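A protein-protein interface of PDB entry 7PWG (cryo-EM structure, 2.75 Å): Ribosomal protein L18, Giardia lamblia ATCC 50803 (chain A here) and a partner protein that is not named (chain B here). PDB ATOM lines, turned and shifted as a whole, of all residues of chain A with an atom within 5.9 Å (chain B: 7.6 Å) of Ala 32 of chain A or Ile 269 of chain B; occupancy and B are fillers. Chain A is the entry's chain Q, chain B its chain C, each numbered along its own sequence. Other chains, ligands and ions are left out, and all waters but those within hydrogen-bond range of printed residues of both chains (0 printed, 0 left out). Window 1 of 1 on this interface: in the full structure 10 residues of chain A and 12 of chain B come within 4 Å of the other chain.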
ATOM      1  N   ARG A  27     -14.258 -24.055  26.589  1.00  0.00           N
ATOM      2  CA  ARG A  27     -15.502 -24.240  25.855  1.00  0.00           C
ATOM      3  C   ARG A  27     -16.445 -23.053  26.041  1.00  0.00           C
ATOM      4  O   ARG A  27     -17.103 -22.625  25.091  1.00  0.00           O
ATOM      5  CB  ARG A  27     -16.192 -25.530  26.292  1.00  0.00           C
ATOM      6  CG  ARG A  27     -15.322 -26.777  26.281  1.00  0.00           C
ATOM      7  CD  ARG A  27     -14.714 -27.022  24.939  1.00  0.00           C
ATOM      8  NE  ARG A  27     -15.591 -27.736  24.017  1.00  0.00           N
ATOM      9  CZ  ARG A  27     -15.486 -29.032  23.739  1.00  0.00           C
ATOM     10  NH1 ARG A  27     -14.547 -29.767  24.323  1.00  0.00           N
ATOM     11  NH2 ARG A  27     -16.318 -29.591  22.877  1.00  0.00           N
ATOM     12  N   LEU A  28     -16.536 -22.518  27.260  1.00  0.00           N
ATOM     13  CA  LEU A  28     -17.454 -21.409  27.501  1.00  0.00           C
ATOM     14  C   LEU A  28     -17.052 -20.165  26.718  1.00  0.00           C
ATOM     15  O   LEU A  28     -17.909 -19.471  26.161  1.00  0.00           O
ATOM     16  CB  LEU A  28     -17.541 -21.091  28.995  1.00  0.00           C
ATOM     17  CG  LEU A  28     -18.179 -22.112  29.944  1.00  0.00           C
ATOM     18  CD1 LEU A  28     -18.378 -21.523  31.325  1.00  0.00           C
ATOM     19  CD2 LEU A  28     -19.483 -22.643  29.407  1.00  0.00           C
ATOM     20  N   LEU A  29     -15.760 -19.851  26.687  1.00  0.00           N
ATOM     21  CA  LEU A  29     -15.307 -18.637  26.016  1.00  0.00           C
ATOM     22  C   LEU A  29     -15.407 -18.758  24.503  1.00  0.00           C
ATOM     23  O   LEU A  29     -15.828 -17.811  23.830  1.00  0.00           O
ATOM     24  CB  LEU A  29     -13.868 -18.326  26.407  1.00  0.00           C
ATOM     25  CG  LEU A  29     -13.531 -17.688  27.736  1.00  0.00           C
ATOM     26  CD1 LEU A  29     -12.040 -17.720  27.847  1.00  0.00           C
ATOM     27  CD2 LEU A  29     -14.027 -16.273  27.747  1.00  0.00           C
ATOM     28  N   HIS A  30     -14.983 -19.896  23.946  1.00  0.00           N
ATOM     29  CA  HIS A  30     -15.075 -20.095  22.505  1.00  0.00           C
ATOM     30  C   HIS A  30     -16.520 -20.064  22.030  1.00  0.00           C
ATOM     31  O   HIS A  30     -16.829 -19.458  21.002  1.00  0.00           O
ATOM     32  CB  HIS A  30     -14.420 -21.415  22.105  1.00  0.00           C
ATOM     33  CG  HIS A  30     -14.820 -21.890  20.747  1.00  0.00           C
ATOM     34  ND1 HIS A  30     -15.884 -22.739  20.540  1.00  0.00           N
ATOM     35  CD2 HIS A  30     -14.318 -21.615  19.524  1.00  0.00           C
ATOM     36  CE1 HIS A  30     -16.022 -22.964  19.249  1.00  0.00           C
ATOM     37  NE2 HIS A  30     -15.082 -22.296  18.611  1.00  0.00           N
ATOM     38  N   ASN A  31     -17.419 -20.723  22.753  1.00  0.00           N
ATOM     39  CA  ASN A  31     -18.822 -20.679  22.371  1.00  0.00           C
ATOM     40  C   ASN A  31     -19.387 -19.267  22.453  1.00  0.00           C
ATOM     41  O   ASN A  31     -20.295 -18.924  21.693  1.00  0.00           O
ATOM     42  CB  ASN A  31     -19.637 -21.622  23.248  1.00  0.00           C
ATOM     43  CG  ASN A  31     -20.073 -22.857  22.512  1.00  0.00           C
ATOM     44  OD1 ASN A  31     -20.439 -22.798  21.343  1.00  0.00           O
ATOM     45  ND2 ASN A  31     -20.024 -23.995  23.189  1.00  0.00           N
ATOM     46  N   ALA A  32     -18.871 -18.441  23.366  1.00  0.00           N
ATOM     47  CA  ALA A  32     -19.356 -17.071  23.494  1.00  0.00           C
ATOM     48  C   ALA A  32     -18.851 -16.169  22.377  1.00  0.00           C
ATOM     49  O   ALA A  32     -19.606 -15.350  21.857  1.00  0.00           O
ATOM     50  CB  ALA A  32     -18.966 -16.500  24.854  1.00  0.00           C
ATOM     51  N   PHE A  33     -17.586 -16.282  21.999  1.00  0.00           N
ATOM     52  CA  PHE A  33     -17.080 -15.417  20.943  1.00  0.00           C
ATOM     53  C   PHE A  33     -17.537 -15.865  19.567  1.00  0.00           C
ATOM     54  O   PHE A  33     -17.629 -15.041  18.654  1.00  0.00           O
ATOM     55  CB  PHE A  33     -15.566 -15.341  21.001  1.00  0.00           C
ATOM     56  CG  PHE A  33     -15.061 -14.327  21.963  1.00  0.00           C
ATOM     57  CD1 PHE A  33     -15.106 -12.991  21.652  1.00  0.00           C
ATOM     58  CD2 PHE A  33     -14.540 -14.701  23.181  1.00  0.00           C
ATOM     59  CE1 PHE A  33     -14.645 -12.053  22.536  1.00  0.00           C
ATOM     60  CE2 PHE A  33     -14.078 -13.755  24.060  1.00  0.00           C
ATOM     61  CZ  PHE A  33     -14.129 -12.439  23.730  1.00  0.00           C
ATOM     62  N   LYS A  34     -17.841 -17.148  19.410  1.00  0.00           N
ATOM     63  CA  LYS A  34     -18.474 -17.634  18.194  1.00  0.00           C
ATOM     64  C   LYS A  34     -19.852 -17.014  17.994  1.00  0.00           C
ATOM     65  O   LYS A  34     -20.265 -16.785  16.855  1.00  0.00           O
ATOM     66  CB  LYS A  34     -18.557 -19.151  18.261  1.00  0.00           C
ATOM     67  CG  LYS A  34     -19.297 -19.818  17.161  1.00  0.00           C
ATOM     68  CD  LYS A  34     -19.348 -21.303  17.414  1.00  0.00           C
ATOM     69  CE  LYS A  34     -19.386 -22.057  16.110  1.00  0.00           C
ATOM     70  NZ  LYS A  34     -20.490 -21.586  15.234  1.00  0.00           N
ATOM     71  N   VAL A  35     -20.566 -16.729  19.083  1.00  0.00           N
ATOM     72  CA  VAL A  35     -21.880 -16.089  18.996  1.00  0.00           C
ATOM     73  C   VAL A  35     -21.749 -14.637  18.552  1.00  0.00           C
ATOM     74  O   VAL A  35     -22.483 -14.167  17.678  1.00  0.00           O
ATOM     75  CB  VAL A  35     -22.606 -16.192  20.348  1.00  0.00           C
ATOM     76  CG1 VAL A  35     -23.756 -15.217  20.416  1.00  0.00           C
ATOM     77  CG2 VAL A  35     -23.090 -17.598  20.578  1.00  0.00           C
ATOM     78  N   VAL A  36     -20.812 -13.905  19.149  1.00  0.00           N
ATOM     79  CA  VAL A  36     -20.643 -12.494  18.824  1.00  0.00           C
ATOM     80  C   VAL A  36     -20.268 -12.317  17.360  1.00  0.00           C
ATOM     81  O   VAL A  36     -20.715 -11.369  16.705  1.00  0.00           O
ATOM     82  CB  VAL A  36     -19.611 -11.848  19.765  1.00  0.00           C
ATOM     83  CG1 VAL A  36     -18.982 -10.642  19.126  1.00  0.00           C
ATOM     84  CG2 VAL A  36     -20.276 -11.446  21.056  1.00  0.00           C
ATOM     85  N   TYR A  37     -19.457 -13.226  16.814  1.00  0.00           N
ATOM     86  CA  TYR A  37     -19.110 -13.130  15.400  1.00  0.00           C
ATOM     87  C   TYR A  37     -20.348 -13.248  14.517  1.00  0.00           C
ATOM     88  O   TYR A  37     -20.514 -12.479  13.565  1.00  0.00           O
ATOM     89  CB  TYR A  37     -18.075 -14.191  15.013  1.00  0.00           C
ATOM     90  CG  TYR A  37     -17.813 -14.192  13.529  1.00  0.00           C
ATOM     91  CD1 TYR A  37     -17.113 -13.160  12.940  1.00  0.00           C
ATOM     92  CD2 TYR A  37     -18.311 -15.190  12.710  1.00  0.00           C
ATOM     93  CE1 TYR A  37     -16.893 -13.125  11.593  1.00  0.00           C
ATOM     94  CE2 TYR A  37     -18.094 -15.161  11.348  1.00  0.00           C
ATOM     95  CZ  TYR A  37     -17.378 -14.125  10.799  1.00  0.00           C
ATOM     96  OH  TYR A  37     -17.146 -14.077   9.445  1.00  0.00           O
ATOM     97  N   ASP A 123     -12.957 -12.858  29.656  1.00  0.00           N
ATOM     98  CA  ASP A 123     -14.341 -12.544  29.968  1.00  0.00           C
ATOM     99  C   ASP A 123     -14.524 -11.094  30.396  1.00  0.00           C
ATOM    100  O   ASP A 123     -15.624 -10.555  30.260  1.00  0.00           O
ATOM    101  CB  ASP A 123     -14.880 -13.492  31.042  1.00  0.00           C
ATOM    102  CG  ASP A 123     -14.089 -13.439  32.324  1.00  0.00           C
ATOM    103  OD1 ASP A 123     -12.868 -13.221  32.258  1.00  0.00           O
ATOM    104  OD2 ASP A 123     -14.682 -13.623  33.400  1.00  0.00           O
ATOM    105  N   LEU A 126     -14.673  -9.708  26.942  1.00  0.00           N
ATOM    106  CA  LEU A 126     -15.957  -9.981  26.317  1.00  0.00           C
ATOM    107  C   LEU A 126     -17.007  -8.971  26.751  1.00  0.00           C
ATOM    108  O   LEU A 126     -17.822  -8.526  25.937  1.00  0.00           O
ATOM    109  CB  LEU A 126     -16.409 -11.398  26.654  1.00  0.00           C
ATOM    110  CG  LEU A 126     -17.748 -11.823  26.059  1.00  0.00           C
ATOM    111  CD1 LEU A 126     -17.545 -12.598  24.775  1.00  0.00           C
ATOM    112  CD2 LEU A 126     -18.570 -12.607  27.063  1.00  0.00           C
ATOM    113  N   ILE B 264     -15.242 -17.704  36.129  1.00  0.00           N
ATOM    114  CA  ILE B 264     -16.683 -17.537  35.983  1.00  0.00           C
ATOM    115  C   ILE B 264     -17.313 -18.816  35.458  1.00  0.00           C
ATOM    116  O   ILE B 264     -16.616 -19.719  34.982  1.00  0.00           O
ATOM    117  CB  ILE B 264     -17.033 -16.355  35.067  1.00  0.00           C
ATOM    118  CG1 ILE B 264     -16.527 -16.618  33.655  1.00  0.00           C
ATOM    119  CG2 ILE B 264     -16.469 -15.064  35.612  1.00  0.00           C
ATOM    120  CD1 ILE B 264     -16.977 -15.589  32.724  1.00  0.00           C
ATOM    121  N   THR B 265     -18.634 -18.900  35.551  1.00  0.00           N
ATOM    122  CA  THR B 265     -19.404 -20.059  35.138  1.00  0.00           C
ATOM    123  C   THR B 265     -20.258 -19.725  33.921  1.00  0.00           C
ATOM    124  O   THR B 265     -20.360 -18.576  33.490  1.00  0.00           O
ATOM    125  CB  THR B 265     -20.280 -20.545  36.294  1.00  0.00           C
ATOM    126  OG1 THR B 265     -19.640 -20.227  37.534  1.00  0.00           O
ATOM    127  CG2 THR B 265     -20.477 -22.039  36.229  1.00  0.00           C
ATOM    128  N   GLN B 266     -20.885 -20.759  33.361  1.00  0.00           N
ATOM    129  CA  GLN B 266     -21.785 -20.548  32.237  1.00  0.00           C
ATOM    130  C   GLN B 266     -23.008 -19.737  32.634  1.00  0.00           C
ATOM    131  O   GLN B 266     -23.663 -19.156  31.764  1.00  0.00           O
ATOM    132  CB  GLN B 266     -22.201 -21.890  31.652  1.00  0.00           C
ATOM    133  CG  GLN B 266     -22.866 -21.801  30.310  1.00  0.00           C
ATOM    134  CD  GLN B 266     -24.259 -22.324  30.358  1.00  0.00           C
ATOM    135  OE1 GLN B 266     -24.684 -22.870  31.373  1.00  0.00           O
ATOM    136  NE2 GLN B 266     -24.996 -22.159  29.266  1.00  0.00           N
ATOM    137  N   THR B 267     -23.335 -19.693  33.925  1.00  0.00           N
ATOM    138  CA  THR B 267     -24.331 -18.743  34.403  1.00  0.00           C
ATOM    139  C   THR B 267     -23.859 -17.311  34.195  1.00  0.00           C
ATOM    140  O   THR B 267     -24.643 -16.438  33.809  1.00  0.00           O
ATOM    141  CB  THR B 267     -24.628 -18.994  35.881  1.00  0.00           C
ATOM    142  OG1 THR B 267     -25.296 -20.250  36.026  1.00  0.00           O
ATOM    143  CG2 THR B 267     -25.493 -17.870  36.458  1.00  0.00           C
ATOM    144  N   ASP B 268     -22.574 -17.061  34.439  1.00  0.00           N
ATOM    145  CA  ASP B 268     -22.031 -15.717  34.323  1.00  0.00           C
ATOM    146  C   ASP B 268     -21.863 -15.295  32.867  1.00  0.00           C
ATOM    147  O   ASP B 268     -22.047 -14.121  32.542  1.00  0.00           O
ATOM    148  CB  ASP B 268     -20.701 -15.630  35.069  1.00  0.00           C
ATOM    149  CG  ASP B 268     -20.818 -16.040  36.532  1.00  0.00           C
ATOM    150  OD1 ASP B 268     -21.807 -16.707  36.903  1.00  0.00           O
ATOM    151  OD2 ASP B 268     -19.914 -15.695  37.318  1.00  0.00           O
ATOM    152  N   ILE B 269     -21.495 -16.225  31.983  1.00  0.00           N
ATOM    153  CA  ILE B 269     -21.328 -15.889  30.569  1.00  0.00           C
ATOM    154  C   ILE B 269     -22.678 -15.606  29.930  1.00  0.00           C
ATOM    155  O   ILE B 269     -22.815 -14.697  29.101  1.00  0.00           O
ATOM    156  CB  ILE B 269     -20.601 -17.014  29.810  1.00  0.00           C
ATOM    157  CG1 ILE B 269     -19.166 -17.205  30.302  1.00  0.00           C
ATOM    158  CG2 ILE B 269     -20.590 -16.715  28.336  1.00  0.00           C
ATOM    159  CD1 ILE B 269     -18.160 -16.334  29.586  1.00  0.00           C
ATOM    160  N   GLU B 270     -23.694 -16.389  30.292  1.00  0.00           N
ATOM    161  CA  GLU B 270     -25.008 -16.194  29.706  1.00  0.00           C
ATOM    162  C   GLU B 270     -25.615 -14.856  30.105  1.00  0.00           C
ATOM    163  O   GLU B 270     -26.505 -14.358  29.409  1.00  0.00           O
ATOM    164  CB  GLU B 270     -25.919 -17.342  30.116  1.00  0.00           C
ATOM    165  CG  GLU B 270     -27.202 -17.443  29.324  1.00  0.00           C
ATOM    166  CD  GLU B 270     -28.363 -17.860  30.189  1.00  0.00           C
ATOM    167  OE1 GLU B 270     -28.269 -17.667  31.416  1.00  0.00           O
ATOM    168  OE2 GLU B 270     -29.361 -18.384  29.648  1.00  0.00           O
ATOM    169  N   ARG B 271     -25.159 -14.276  31.214  1.00  0.00           N
ATOM    170  CA  ARG B 271     -25.655 -12.971  31.639  1.00  0.00           C
ATOM    171  C   ARG B 271     -25.079 -11.856  30.780  1.00  0.00           C
ATOM    172  O   ARG B 271     -25.790 -10.915  30.414  1.00  0.00           O
ATOM    173  CB  ARG B 271     -25.307 -12.736  33.107  1.00  0.00           C
ATOM    174  CG  ARG B 271     -25.599 -11.330  33.593  1.00  0.00           C
ATOM    175  CD  ARG B 271     -25.033 -11.073  34.979  1.00  0.00           C
ATOM    176  NE  ARG B 271     -23.801 -10.288  34.932  1.00  0.00           N
ATOM    177  CZ  ARG B 271     -22.582 -10.782  35.128  1.00  0.00           C
ATOM    178  NH1 ARG B 271     -21.528  -9.983  35.059  1.00  0.00           N
ATOM    179  NH2 ARG B 271     -22.414 -12.068  35.398  1.00  0.00           N
ATOM    180  N   ILE B 272     -23.790 -11.944  30.456  1.00  0.00           N
ATOM    181  CA  ILE B 272     -23.112 -10.836  29.799  1.00  0.00           C
ATOM    182  C   ILE B 272     -23.685 -10.604  28.409  1.00  0.00           C
ATOM    183  O   ILE B 272     -23.962  -9.466  28.020  1.00  0.00           O
ATOM    184  CB  ILE B 272     -21.595 -11.084  29.746  1.00  0.00           C
ATOM    185  CG1 ILE B 272     -21.088 -11.639  31.070  1.00  0.00           C
ATOM    186  CG2 ILE B 272     -20.900  -9.804  29.487  1.00  0.00           C
ATOM    187  CD1 ILE B 272     -19.586 -11.806  31.143  1.00  0.00           C
ATOM    188  N   LEU B 273     -23.870 -11.677  27.641  1.00  0.00           N
ATOM    189  CA  LEU B 273     -24.354 -11.543  26.274  1.00  0.00           C
ATOM    190  C   LEU B 273     -25.710 -10.857  26.208  1.00  0.00           C
ATOM    191  O   LEU B 273     -26.023 -10.196  25.214  1.00  0.00           O
ATOM    192  CB  LEU B 273     -24.448 -12.915  25.620  1.00  0.00           C
ATOM    193  CG  LEU B 273     -23.133 -13.635  25.350  1.00  0.00           C
ATOM    194  CD1 LEU B 273     -23.435 -15.026  24.857  1.00  0.00           C
ATOM    195  CD2 LEU B 273     -22.309 -12.862  24.337  1.00  0.00           C
ATOM    196  N   GLN B 274     -26.534 -11.032  27.232  1.00  0.00           N
ATOM    197  CA  GLN B 274     -27.853 -10.415  27.299  1.00  0.00           C
ATOM    198  C   GLN B 274     -27.801  -9.085  28.044  1.00  0.00           C
ATOM    199  O   GLN B 274     -28.609  -8.806  28.926  1.00  0.00           O
ATOM    200  CB  GLN B 274     -28.829 -11.380  27.959  1.00  0.00           C
ATOM    201  CG  GLN B 274     -29.628 -12.236  26.993  1.00  0.00           C
ATOM    202  CD  GLN B 274     -28.829 -13.355  26.350  1.00  0.00           C
ATOM    203  OE1 GLN B 274     -28.634 -13.371  25.138  1.00  0.00           O
ATOM    204  NE2 GLN B 274     -28.394 -14.318  27.157  1.00  0.00           N
ATOM    205  N   VAL B 278     -23.030  -5.544  25.124  1.00  0.00           N
ATOM    206  CA  VAL B 278     -22.808  -6.518  24.059  1.00  0.00           C
ATOM    207  C   VAL B 278     -23.905  -6.450  23.004  1.00  0.00           C
ATOM    208  O   VAL B 278     -23.632  -6.571  21.809  1.00  0.00           O
ATOM    209  CB  VAL B 278     -22.704  -7.933  24.665  1.00  0.00           C
ATOM    210  CG1 VAL B 278     -21.999  -8.894  23.706  1.00  0.00           C
ATOM    211  CG2 VAL B 278     -22.004  -7.891  26.009  1.00  0.00           C
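Among the printed residues, merely in contact across the chains: Asp 123 of chain A with Ile 264 of chain B (3.1 Å), Leu 28 of chain A with Gln 266 of chain B (3.3 Å), Leu 28 of chain A with Thr 265 of chain B (3.7 Å) and Ala 32 of chain A with Ile 269 of chain B (3.8 Å).
Ala 32 of chain A touches just one residue of chain B: Ile 269. Of the printed residues of chain A, Thr 265 of chain B touches Leu 28. Of the printed residues of chain A, Ile 264 of chain B touches Asp 123 (3.1 Å). The nearest residue of chain B that does not touch Ala 32 of chain A is Leu 273 of chain B (4.4 Å). The nearest residue of chain A that does not touch Ile 269 of chain B is Leu 28 of chain A (4.4 Å).
Printed residues of chain B that touch a printed residue of chain A: Ile 264, Thr 265, Gln 266 and Ile 269. Hydrophobic or aromatic side chains of chain B that line the printed part of chain A: Ile 264 and Ile 269. Of the 13 printed residues of chain A, 3 touch a printed residue of chain B. Among the printed residues, 4 pairs touch across the chains. Among the printed residues, no Asp or Glu carboxylate lies within 4 Å of a Lys or Arg side-chain nitrogen of the other chain.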
